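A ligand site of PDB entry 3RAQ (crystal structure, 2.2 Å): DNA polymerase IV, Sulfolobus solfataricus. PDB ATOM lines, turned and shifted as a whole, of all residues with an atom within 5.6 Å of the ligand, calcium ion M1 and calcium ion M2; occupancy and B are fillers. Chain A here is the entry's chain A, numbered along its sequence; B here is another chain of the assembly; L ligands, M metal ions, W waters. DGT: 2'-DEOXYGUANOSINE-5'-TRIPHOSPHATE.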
ATOM      1  N   ASP A   7      34.532  -1.624  22.844  1.00  0.00           N
ATOM      2  CA  ASP A   7      33.515  -2.589  22.373  1.00  0.00           C
ATOM      3  C   ASP A   7      32.957  -3.398  23.541  1.00  0.00           C
ATOM      4  O   ASP A   7      33.732  -4.080  24.212  1.00  0.00           O
ATOM      5  CB  ASP A   7      34.118  -3.584  21.363  1.00  0.00           C
ATOM      6  CG  ASP A   7      33.165  -4.715  21.035  1.00  0.00           C
ATOM      7  OD1 ASP A   7      33.278  -5.830  21.634  1.00  0.00           O
ATOM      8  OD2 ASP A   7      32.250  -4.464  20.236  1.00  0.00           O
ATOM      9  N   PHE A   8      31.644  -3.360  23.764  1.00  0.00           N
ATOM     10  CA  PHE A   8      31.028  -3.998  24.940  1.00  0.00           C
ATOM     11  C   PHE A   8      31.029  -5.511  24.795  1.00  0.00           C
ATOM     12  O   PHE A   8      30.728  -6.021  23.729  1.00  0.00           O
ATOM     13  CB  PHE A   8      29.589  -3.503  25.169  1.00  0.00           C
ATOM     14  CG  PHE A   8      29.419  -1.991  25.043  1.00  0.00           C
ATOM     15  CD1 PHE A   8      30.462  -1.107  25.305  1.00  0.00           C
ATOM     16  CD2 PHE A   8      28.190  -1.474  24.695  1.00  0.00           C
ATOM     17  CE1 PHE A   8      30.284   0.252  25.177  1.00  0.00           C
ATOM     18  CE2 PHE A   8      27.995  -0.116  24.582  1.00  0.00           C
ATOM     19  CZ  PHE A   8      29.043   0.750  24.829  1.00  0.00           C
ATOM     20  N   ASP A   9      31.402  -6.240  25.847  1.00  0.00           N
ATOM     21  CA  ASP A   9      31.510  -7.713  25.748  1.00  0.00           C
ATOM     22  C   ASP A   9      30.119  -8.375  25.688  1.00  0.00           C
ATOM     23  O   ASP A   9      29.202  -7.998  26.424  1.00  0.00           O
ATOM     24  CB  ASP A   9      32.304  -8.305  26.914  1.00  0.00           C
ATOM     25  CG  ASP A   9      33.737  -7.746  27.021  1.00  0.00           C
ATOM     26  OD1 ASP A   9      34.332  -7.344  26.007  1.00  0.00           O
ATOM     27  OD2 ASP A   9      34.268  -7.721  28.164  1.00  0.00           O
ATOM     28  N   TYR A  10      29.993  -9.388  24.814  1.00  0.00           N
ATOM     29  CA  TYR A  10      28.755 -10.163  24.573  1.00  0.00           C
ATOM     30  C   TYR A  10      27.470  -9.394  24.872  1.00  0.00           C
ATOM     31  O   TYR A  10      26.605  -9.841  25.630  1.00  0.00           O
ATOM     32  CB  TYR A  10      28.804 -11.537  25.283  1.00  0.00           C
ATOM     33  CG  TYR A  10      28.936 -11.524  26.800  1.00  0.00           C
ATOM     34  CD1 TYR A  10      27.867 -11.885  27.616  1.00  0.00           C
ATOM     35  CD2 TYR A  10      30.147 -11.190  27.411  1.00  0.00           C
ATOM     36  CE1 TYR A  10      27.967 -11.891  29.005  1.00  0.00           C
ATOM     37  CE2 TYR A  10      30.267 -11.199  28.823  1.00  0.00           C
ATOM     38  CZ  TYR A  10      29.174 -11.543  29.600  1.00  0.00           C
ATOM     39  OH  TYR A  10      29.283 -11.559  30.985  1.00  0.00           O
ATOM     40  N   PHE A  11      27.353  -8.231  24.225  1.00  0.00           N
ATOM     41  CA  PHE A  11      26.553  -7.132  24.763  1.00  0.00           C
ATOM     42  C   PHE A  11      25.131  -7.500  25.191  1.00  0.00           C
ATOM     43  O   PHE A  11      24.778  -7.298  26.353  1.00  0.00           O
ATOM     44  CB  PHE A  11      26.534  -5.938  23.813  1.00  0.00           C
ATOM     45  CG  PHE A  11      25.813  -4.742  24.367  1.00  0.00           C
ATOM     46  CD1 PHE A  11      26.078  -4.294  25.661  1.00  0.00           C
ATOM     47  CD2 PHE A  11      24.878  -4.060  23.613  1.00  0.00           C
ATOM     48  CE1 PHE A  11      25.422  -3.199  26.193  1.00  0.00           C
ATOM     49  CE2 PHE A  11      24.202  -2.968  24.135  1.00  0.00           C
ATOM     50  CZ  PHE A  11      24.488  -2.534  25.431  1.00  0.00           C
ATOM     51  N   TYR A  12      24.305  -8.018  24.270  1.00  0.00           N
ATOM     52  CA  TYR A  12      22.872  -8.244  24.600  1.00  0.00           C
ATOM     53  C   TYR A  12      22.730  -9.265  25.712  1.00  0.00           C
ATOM     54  O   TYR A  12      21.942  -9.092  26.622  1.00  0.00           O
ATOM     55  CB  TYR A  12      22.055  -8.711  23.407  1.00  0.00           C
ATOM     56  CG  TYR A  12      21.860  -7.732  22.258  1.00  0.00           C
ATOM     57  CD1 TYR A  12      22.427  -6.459  22.260  1.00  0.00           C
ATOM     58  CD2 TYR A  12      21.117  -8.123  21.141  1.00  0.00           C
ATOM     59  CE1 TYR A  12      22.239  -5.591  21.200  1.00  0.00           C
ATOM     60  CE2 TYR A  12      20.926  -7.262  20.070  1.00  0.00           C
ATOM     61  CZ  TYR A  12      21.487  -6.000  20.106  1.00  0.00           C
ATOM     62  OH  TYR A  12      21.305  -5.165  19.023  1.00  0.00           O
ATOM     63  N   ALA A  13      23.475 -10.363  25.619  1.00  0.00           N
ATOM     64  CA  ALA A  13      23.445 -11.370  26.670  1.00  0.00           C
ATOM     65  C   ALA A  13      23.927 -10.796  27.998  1.00  0.00           C
ATOM     66  O   ALA A  13      23.417 -11.167  29.036  1.00  0.00           O
ATOM     67  CB  ALA A  13      24.275 -12.625  26.279  1.00  0.00           C
ATOM     68  N   VAL A  32      16.021 -14.200  18.386  1.00  0.00           N
ATOM     69  CA  VAL A  32      14.920 -13.602  17.659  1.00  0.00           C
ATOM     70  C   VAL A  32      14.030 -14.728  17.178  1.00  0.00           C
ATOM     71  O   VAL A  32      14.366 -15.415  16.219  1.00  0.00           O
ATOM     72  CB  VAL A  32      15.416 -12.753  16.484  1.00  0.00           C
ATOM     73  CG1 VAL A  32      14.256 -11.964  15.875  1.00  0.00           C
ATOM     74  CG2 VAL A  32      16.495 -11.800  16.944  1.00  0.00           C
ATOM     75  N   VAL A  43      19.815 -17.018  16.639  1.00  0.00           N
ATOM     76  CA  VAL A  43      20.479 -16.466  17.813  1.00  0.00           C
ATOM     77  C   VAL A  43      21.044 -15.088  17.465  1.00  0.00           C
ATOM     78  O   VAL A  43      21.778 -14.944  16.484  1.00  0.00           O
ATOM     79  CB  VAL A  43      21.628 -17.401  18.268  1.00  0.00           C
ATOM     80  CG1 VAL A  43      22.468 -16.764  19.385  1.00  0.00           C
ATOM     81  CG2 VAL A  43      21.071 -18.758  18.696  1.00  0.00           C
ATOM     82  N   ALA A  44      20.711 -14.059  18.249  1.00  0.00           N
ATOM     83  CA  ALA A  44      21.308 -12.733  18.057  1.00  0.00           C
ATOM     84  C   ALA A  44      22.685 -12.698  18.667  1.00  0.00           C
ATOM     85  O   ALA A  44      23.647 -12.165  18.076  1.00  0.00           O
ATOM     86  CB  ALA A  44      20.444 -11.637  18.677  1.00  0.00           C
ATOM     87  N   THR A  45      22.794 -13.264  19.865  1.00  0.00           N
ATOM     88  CA  THR A  45      24.088 -13.422  20.515  1.00  0.00           C
ATOM     89  C   THR A  45      23.994 -14.353  21.710  1.00  0.00           C
ATOM     90  O   THR A  45      22.914 -14.617  22.219  1.00  0.00           O
ATOM     91  CB  THR A  45      24.693 -12.079  20.956  1.00  0.00           C
ATOM     92  OG1 THR A  45      26.062 -12.276  21.285  1.00  0.00           O
ATOM     93  CG2 THR A  45      23.973 -11.474  22.163  1.00  0.00           C
ATOM     94  N   ALA A  46      25.125 -14.863  22.143  1.00  0.00           N
ATOM     95  CA  ALA A  46      25.181 -15.727  23.318  1.00  0.00           C
ATOM     96  C   ALA A  46      26.338 -15.279  24.185  1.00  0.00           C
ATOM     97  O   ALA A  46      27.233 -14.621  23.689  1.00  0.00           O
ATOM     98  CB  ALA A  46      25.343 -17.167  22.893  1.00  0.00           C
ATOM     99  N   TYR A  48      29.761 -16.143  26.625  1.00  0.00           N
ATOM    100  CA  TYR A  48      30.940 -16.975  26.356  1.00  0.00           C
ATOM    101  C   TYR A  48      30.792 -18.420  26.832  1.00  0.00           C
ATOM    102  O   TYR A  48      31.349 -19.326  26.214  1.00  0.00           O
ATOM    103  CB  TYR A  48      32.214 -16.318  26.910  1.00  0.00           C
ATOM    104  CG  TYR A  48      32.708 -15.254  25.969  1.00  0.00           C
ATOM    105  CD1 TYR A  48      32.069 -14.019  25.887  1.00  0.00           C
ATOM    106  CD2 TYR A  48      33.790 -15.498  25.112  1.00  0.00           C
ATOM    107  CE1 TYR A  48      32.489 -13.033  24.985  1.00  0.00           C
ATOM    108  CE2 TYR A  48      34.219 -14.522  24.206  1.00  0.00           C
ATOM    109  CZ  TYR A  48      33.558 -13.286  24.148  1.00  0.00           C
ATOM    110  OH  TYR A  48      33.962 -12.307  23.273  1.00  0.00           O
ATOM    111  N   ARG A  51      29.027 -19.911  23.893  1.00  0.00           N
ATOM    112  CA  ARG A  51      29.940 -19.967  22.753  1.00  0.00           C
ATOM    113  C   ARG A  51      30.934 -21.107  22.787  1.00  0.00           C
ATOM    114  O   ARG A  51      31.391 -21.550  21.727  1.00  0.00           O
ATOM    115  CB  ARG A  51      30.718 -18.669  22.639  1.00  0.00           C
ATOM    116  CG  ARG A  51      29.869 -17.543  22.142  1.00  0.00           C
ATOM    117  CD  ARG A  51      30.680 -16.293  21.952  1.00  0.00           C
ATOM    118  NE  ARG A  51      29.863 -15.111  22.161  1.00  0.00           N
ATOM    119  CZ  ARG A  51      30.219 -13.873  21.820  1.00  0.00           C
ATOM    120  NH1 ARG A  51      31.389 -13.649  21.240  1.00  0.00           N
ATOM    121  NH2 ARG A  51      29.376 -12.873  22.060  1.00  0.00           N
ATOM    122  N   ALA A  57      26.143 -15.982  17.426  1.00  0.00           N
ATOM    123  CA  ALA A  57      25.327 -15.118  16.550  1.00  0.00           C
ATOM    124  C   ALA A  57      25.127 -15.797  15.197  1.00  0.00           C
ATOM    125  O   ALA A  57      26.086 -16.234  14.567  1.00  0.00           O
ATOM    126  CB  ALA A  57      25.988 -13.749  16.380  1.00  0.00           C
ATOM    127  N   GLY A  58      23.875 -15.908  14.774  1.00  0.00           N
ATOM    128  CA  GLY A  58      23.559 -16.318  13.410  1.00  0.00           C
ATOM    129  C   GLY A  58      23.106 -17.759  13.232  1.00  0.00           C
ATOM    130  O   GLY A  58      22.529 -18.085  12.197  1.00  0.00           O
ATOM    131  N   MET A  76      15.087 -11.350  22.213  1.00  0.00           N
ATOM    132  CA  MET A  76      15.796 -10.099  22.028  1.00  0.00           C
ATOM    133  C   MET A  76      14.915  -8.906  22.396  1.00  0.00           C
ATOM    134  O   MET A  76      13.892  -8.702  21.784  1.00  0.00           O
ATOM    135  CB  MET A  76      16.258  -9.942  20.569  1.00  0.00           C
ATOM    136  CG  MET A  76      17.295  -8.861  20.353  1.00  0.00           C
ATOM    137  SD  MET A  76      17.808  -8.663  18.634  1.00  0.00           S
ATOM    138  CE  MET A  76      16.313  -7.977  17.889  1.00  0.00           C
ATOM    139  N   SER A 103      28.616   1.400  16.291  1.00  0.00           N
ATOM    140  CA  SER A 103      27.571   0.394  16.346  1.00  0.00           C
ATOM    141  C   SER A 103      26.793   0.544  17.636  1.00  0.00           C
ATOM    142  O   SER A 103      27.067   1.428  18.446  1.00  0.00           O
ATOM    143  CB  SER A 103      28.148  -1.038  16.271  1.00  0.00           C
ATOM    144  OG  SER A 103      28.562  -1.499  17.544  1.00  0.00           O
ATOM    145  N   ILE A 104      25.833  -0.337  17.853  1.00  0.00           N
ATOM    146  CA  ILE A 104      25.073  -0.358  19.102  1.00  0.00           C
ATOM    147  C   ILE A 104      25.943  -0.655  20.338  1.00  0.00           C
ATOM    148  O   ILE A 104      25.497  -0.423  21.457  1.00  0.00           O
ATOM    149  CB  ILE A 104      23.892  -1.391  19.023  1.00  0.00           C
ATOM    150  CG1 ILE A 104      22.993  -1.247  20.275  1.00  0.00           C
ATOM    151  CG2 ILE A 104      24.442  -2.801  18.872  1.00  0.00           C
ATOM    152  CD1 ILE A 104      21.551  -1.636  20.076  1.00  0.00           C
ATOM    153  N   ASP A 105      27.156  -1.171  20.147  1.00  0.00           N
ATOM    154  CA  ASP A 105      28.020  -1.535  21.282  1.00  0.00           C
ATOM    155  C   ASP A 105      29.485  -1.112  21.162  1.00  0.00           C
ATOM    156  O   ASP A 105      30.337  -1.648  21.872  1.00  0.00           O
ATOM    157  CB  ASP A 105      27.914  -3.056  21.568  1.00  0.00           C
ATOM    158  CG  ASP A 105      28.957  -3.884  20.812  1.00  0.00           C
ATOM    159  OD1 ASP A 105      29.326  -3.553  19.643  1.00  0.00           O
ATOM    160  OD2 ASP A 105      29.403  -4.894  21.407  1.00  0.00           O
ATOM    161  N   GLU A 106      29.799  -0.151  20.292  1.00  0.00           N
ATOM    162  CA  GLU A 106      31.196   0.275  20.148  1.00  0.00           C
ATOM    163  C   GLU A 106      31.355   1.727  19.698  1.00  0.00           C
ATOM    164  O   GLU A 106      30.520   2.275  18.994  1.00  0.00           O
ATOM    165  CB  GLU A 106      31.963  -0.664  19.208  1.00  0.00           C
ATOM    166  CG  GLU A 106      31.734  -0.440  17.721  1.00  0.00           C
ATOM    167  CD  GLU A 106      32.115  -1.631  16.864  1.00  0.00           C
ATOM    168  OE1 GLU A 106      32.897  -1.433  15.893  1.00  0.00           O
ATOM    169  OE2 GLU A 106      31.665  -2.765  17.165  1.00  0.00           O
ATOM    170  N   LYS A 152      41.137  -0.799  16.718  1.00  0.00           N
ATOM    171  CA  LYS A 152      40.228  -1.923  16.503  1.00  0.00           C
ATOM    172  C   LYS A 152      40.958  -3.259  16.634  1.00  0.00           C
ATOM    173  O   LYS A 152      40.506  -4.160  17.348  1.00  0.00           O
ATOM    174  CB  LYS A 152      39.601  -1.798  15.123  1.00  0.00           C
ATOM    175  CG  LYS A 152      38.625  -2.905  14.743  1.00  0.00           C
ATOM    176  CD  LYS A 152      37.319  -2.753  15.448  1.00  0.00           C
ATOM    177  CE  LYS A 152      36.353  -3.840  14.999  1.00  0.00           C
ATOM    178  NZ  LYS A 152      35.194  -3.913  15.940  1.00  0.00           N
ATOM    179  N   LYS A 159      40.000  -9.045  23.523  1.00  0.00           N
ATOM    180  CA  LYS A 159      38.673  -9.447  24.032  1.00  0.00           C
ATOM    181  C   LYS A 159      38.666 -10.919  24.484  1.00  0.00           C
ATOM    182  O   LYS A 159      39.472 -11.717  24.025  1.00  0.00           O
ATOM    183  CB  LYS A 159      37.522  -9.095  23.063  1.00  0.00           C
ATOM    184  CG  LYS A 159      37.546  -9.749  21.704  1.00  0.00           C
ATOM    185  CD  LYS A 159      36.222  -9.505  20.938  1.00  0.00           C
ATOM    186  CE  LYS A 159      36.005  -8.057  20.491  1.00  0.00           C
ATOM    187  NZ  LYS A 159      34.713  -7.829  19.734  1.00  0.00           N
ATOM    188  N   PRO A 160      37.814 -11.259  25.464  1.00  0.00           N
ATOM    189  CA  PRO A 160      36.914 -10.398  26.216  1.00  0.00           C
ATOM    190  C   PRO A 160      37.557  -9.775  27.454  1.00  0.00           C
ATOM    191  O   PRO A 160      38.638 -10.178  27.858  1.00  0.00           O
ATOM    192  CB  PRO A 160      35.805 -11.371  26.643  1.00  0.00           C
ATOM    193  CG  PRO A 160      36.546 -12.663  26.873  1.00  0.00           C
ATOM    194  CD  PRO A 160      37.802 -12.634  25.993  1.00  0.00           C
ATOM    195  P    DC B   6      15.837 -16.003   9.116  1.00  0.00           P
ATOM    196  OP1  DC B   6      14.619 -16.850   9.100  1.00  0.00           O
ATOM    197  OP2  DC B   6      16.391 -15.422   7.865  1.00  0.00           O
ATOM    198  O5'  DC B   6      15.603 -14.867  10.202  1.00  0.00           O
ATOM    199  C5'  DC B   6      14.741 -15.119  11.294  1.00  0.00           C
ATOM    200  C4'  DC B   6      14.917 -13.992  12.270  1.00  0.00           C
ATOM    201  O4'  DC B   6      16.268 -14.107  12.777  1.00  0.00           O
ATOM    202  C3'  DC B   6      14.770 -12.605  11.633  1.00  0.00           C
ATOM    203  O3'  DC B   6      14.005 -11.739  12.453  1.00  0.00           O
ATOM    204  C2'  DC B   6      16.208 -12.150  11.457  1.00  0.00           C
ATOM    205  C1'  DC B   6      16.895 -12.860  12.620  1.00  0.00           C
ATOM    206  N1   DC B   6      18.366 -13.045  12.411  1.00  0.00           N
ATOM    207  C2   DC B   6      19.231 -12.463  13.347  1.00  0.00           C
ATOM    208  O2   DC B   6      18.749 -11.845  14.317  1.00  0.00           O
ATOM    209  N3   DC B   6      20.561 -12.611  13.183  1.00  0.00           N
ATOM    210  C4   DC B   6      21.063 -13.284  12.157  1.00  0.00           C
ATOM    211  N4   DC B   6      22.397 -13.366  12.070  1.00  0.00           N
ATOM    212  C5   DC B   6      20.200 -13.886  11.180  1.00  0.00           C
ATOM    213  C6   DC B   6      18.870 -13.744  11.357  1.00  0.00           C
ATOM    214  P   MG1 B   7      13.482 -10.332  11.916  1.00  0.00           P
ATOM    215  OP1 MG1 B   7      12.435  -9.837  12.867  1.00  0.00           O
ATOM    216  OP2 MG1 B   7      13.236 -10.435  10.433  1.00  0.00           O
ATOM    217  O5' MG1 B   7      14.731  -9.358  12.102  1.00  0.00           O
ATOM    218  C5' MG1 B   7      15.099  -8.997  13.413  1.00  0.00           C
ATOM    219  C4' MG1 B   7      16.446  -8.276  13.342  1.00  0.00           C
ATOM    220  O4' MG1 B   7      17.490  -9.167  12.995  1.00  0.00           O
ATOM    221  C3' MG1 B   7      16.496  -7.147  12.318  1.00  0.00           C
ATOM    222  O3' MG1 B   7      16.122  -5.941  12.979  1.00  0.00           O
ATOM    223  C2' MG1 B   7      17.945  -7.145  11.844  1.00  0.00           C
ATOM    224  C1' MG1 B   7      18.556  -8.312  12.597  1.00  0.00           C
ATOM    225  N9  MG1 B   7      19.545  -9.089  11.825  1.00  0.00           N
ATOM    226  C8  MG1 B   7      19.305 -10.050  10.924  1.00  0.00           C
ATOM    227  N7  MG1 B   7      20.495 -10.512  10.477  1.00  0.00           N
ATOM    228  C5  MG1 B   7      21.471  -9.823  11.099  1.00  0.00           C
ATOM    229  C6  MG1 B   7      22.855  -9.849  11.048  1.00  0.00           C
ATOM    230  O6  MG1 B   7      23.416 -10.646  10.278  1.00  0.00           O
ATOM    231  N1  MG1 B   7      23.577  -8.993  11.819  1.00  0.00           N
ATOM    232  CM1 MG1 B   7      25.046  -8.998  11.772  1.00  0.00           C
ATOM    233  C2  MG1 B   7      22.931  -8.131  12.633  1.00  0.00           C
ATOM    234  N2  MG1 B   7      23.599  -7.257  13.419  1.00  0.00           N
ATOM    235  N3  MG1 B   7      21.587  -8.084  12.711  1.00  0.00           N
ATOM    236  C4  MG1 B   7      20.848  -8.920  11.948  1.00  0.00           C
HETATM  237  PG  DGT L   1      31.628  -9.662  21.773  1.00  0.00           P
HETATM  238  O1G DGT L   1      32.199  -8.609  20.852  1.00  0.00           O
HETATM  239  O2G DGT L   1      32.362 -10.204  22.977  1.00  0.00           O
HETATM  240  O3G DGT L   1      32.387 -10.701  20.981  1.00  0.00           O
HETATM  241  O3B DGT L   1      30.240 -10.378  21.337  1.00  0.00           O
HETATM  242  PB  DGT L   1      29.097  -9.311  20.968  1.00  0.00           P
HETATM  243  O1B DGT L   1      29.272  -7.989  21.746  1.00  0.00           O
HETATM  244  O2B DGT L   1      27.776  -9.954  21.286  1.00  0.00           O
HETATM  245  O3A DGT L   1      29.225  -9.147  19.370  1.00  0.00           O
HETATM  246  PA  DGT L   1      29.366  -7.754  18.580  1.00  0.00           P
HETATM  247  O1A DGT L   1      30.303  -6.717  19.176  1.00  0.00           O
HETATM  248  O2A DGT L   1      29.765  -8.153  17.202  1.00  0.00           O
HETATM  249  O5' DGT L   1      27.891  -7.161  18.433  1.00  0.00           O
HETATM  250  C5' DGT L   1      27.288  -6.405  19.479  1.00  0.00           C
HETATM  251  C4' DGT L   1      25.802  -6.715  19.503  1.00  0.00           C
HETATM  252  O4' DGT L   1      25.279  -6.584  18.175  1.00  0.00           O
HETATM  253  C3' DGT L   1      25.518  -8.151  19.918  1.00  0.00           C
HETATM  254  O3' DGT L   1      25.536  -8.329  21.342  1.00  0.00           O
HETATM  255  C2' DGT L   1      24.182  -8.390  19.229  1.00  0.00           C
HETATM  256  C1' DGT L   1      24.223  -7.518  17.975  1.00  0.00           C
HETATM  257  N9  DGT L   1      24.476  -8.493  16.918  1.00  0.00           N
HETATM  258  C8  DGT L   1      25.678  -8.939  16.439  1.00  0.00           C
HETATM  259  N7  DGT L   1      25.564  -9.862  15.537  1.00  0.00           N
HETATM  260  C5  DGT L   1      24.196 -10.044  15.405  1.00  0.00           C
HETATM  261  C6  DGT L   1      23.432 -10.923  14.583  1.00  0.00           C
HETATM  262  O6  DGT L   1      23.856 -11.759  13.775  1.00  0.00           O
HETATM  263  N1  DGT L   1      22.044 -10.784  14.788  1.00  0.00           N
HETATM  264  C2  DGT L   1      21.453  -9.908  15.672  1.00  0.00           C
HETATM  265  N2  DGT L   1      20.127  -9.870  15.785  1.00  0.00           N
HETATM  266  N3  DGT L   1      22.192  -9.088  16.428  1.00  0.00           N
HETATM  267  C4  DGT L   1      23.518  -9.206  16.254  1.00  0.00           C
HETATM  268 CA    CA M   1      30.923  -4.637  18.338  1.00  0.00          CA
HETATM  269 CA    CA M   2      31.053  -6.523  21.497  1.00  0.00          CA
HETATM  270  O   HOH W   1      32.236  -6.018  17.098  1.00  0.00           O
HETATM  271  O   HOH W   2      26.041 -12.436  12.662  1.00  0.00           O
HETATM  272  O   HOH W   3      27.756 -10.856  14.447  1.00  0.00           O
HETATM  273  O   HOH W   4      28.684  -8.312  14.748  1.00  0.00           O
HETATM  274  O   HOH W   5      26.595  -4.898  16.330  1.00  0.00           O
HETATM  275  O   HOH W   6      30.770 -11.685  18.212  1.00  0.00           O
HETATM  276  O   HOH W   7      29.273  -4.431  16.733  1.00  0.00           O
HETATM  277  O   HOH W   8      20.718  -6.660  16.692  1.00  0.00           O
HETATM  278  O   HOH W   9      34.266  -7.921  23.558  1.00  0.00           O
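The backbone carbonyl oxygen (O) of Phe 8 is bound to calcium ion M2 (2.3 Å). Calcium ion M2 is bound by O1B of the ligand (2.3 Å). OD2 of Asp 105 is bound to calcium ion M2 (2.3 Å). OD1 of Asp 7 of chain A binds calcium ion M2 (2.3 Å). Calcium ion M2 is bound by O1A of the ligand (2.4 Å). O1G of the ligand is bound to calcium ion M2, 2.5 Å away. Calcium ion M2 is bound by OD2 of Asp 7 of chain A, 2.7 Å away.
Water W8 lies within hydrogen-bond range of OH of Tyr 12 (2.8 Å) and N3 of the ligand (2.9 Å). Water W9 bridges OD1 of Asp 9 (2.5 Å) and O2G of the ligand (3.0 Å).
The backbone NH (N) of Tyr 10 sits at hydrogen-bond distance from an oxygen (O2G) of the ligand (3.1 Å). N3 of MG1 7 of chain B lies within hydrogen-bond range of a nitrogen (N1) of the ligand, at 3.4 Å. N of Tyr 12 is in hydrogen-bond range of O3' of the ligand (3.2 Å). OH of Tyr 48 sits at hydrogen-bond distance from O2G of the ligand, 2.7 Å away. O3' of the ligand sits at hydrogen-bond distance from N of Phe 11 (3.4 Å). A nitrogen (N2) of the ligand sits at hydrogen-bond distance from O2 of DC 6 of chain B (2.8 Å). NH1 of Arg 51 is in salt-bridge range of O3G of the ligand, at 3.1 Å. An oxygen (O2B) of the ligand sits at hydrogen-bond distance from the side-chain hydroxyl (OG1) of Thr 45 (2.9 Å). The side-chain amino group (NZ) of Lys 159 is in salt-bridge range of an oxygen (O3G) of the ligand, at 3.9 Å.
Asp 9 touches the ligand. Ala 44 touches the ligand (CB to N2, 3.4 Å). Ala 57 touches the ligand (CB to O6, 3.9 Å). Met 76 touches the ligand. Ile 104 touches the ligand. Hydrophobic or aromatic side chains within 4 Å of the ligand: Phe 11, Tyr 12, Ala 44, Tyr 48, Ala 57, Met 76 and Ile 104.
The side-chain amino group (NZ) of Lys 159 sits close to the side-chain carboxylate (OD1) of Asp 7 of chain A, 3.1 Å away. The side-chain hydroxyl of Thr 45 sits at hydrogen-bond distance from the guanidinium group of Arg 51 (3.5 Å). The guanidinium group of Arg 51 lies within hydrogen-bond range of the backbone carbonyl oxygen of Ala 46. The backbone NH (N) of Glu 106 is in hydrogen-bond range of the side-chain hydroxyl (OG) of Ser 103. The side-chain amino group (NZ) of Lys 152 is in salt-bridge range of the side-chain carboxylate (OE1) of Glu 106 (3.4 Å). The backbone NH of Asp 105 sits at hydrogen-bond distance from the side-chain hydroxyl of Ser 103 (3.0 Å).
Calcium ion M1 is bound by water W1, water W7, OD2 of Asp 7 of chain A, O1A of the ligand, OD1 of Asp 105 and OE2 of Glu 106. Calcium ion M1 has six donor atoms within binding distance.
Within 4 Å of calcium ion M2: Asp 7 of chain A, Phe 8 and Asp 105. Along chain A the residues within 4 Å of calcium ion M2 span positions 7 to 105.
Within 4 Å of calcium ion M1: Asp 7 of chain A, Asp 105 and Glu 106. Along chain A the residues within 4 Å of calcium ion M1 span positions 7 to 106. The nearest printed residue that does not touch calcium ion M1 is Ser 103 (4.01 Å).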
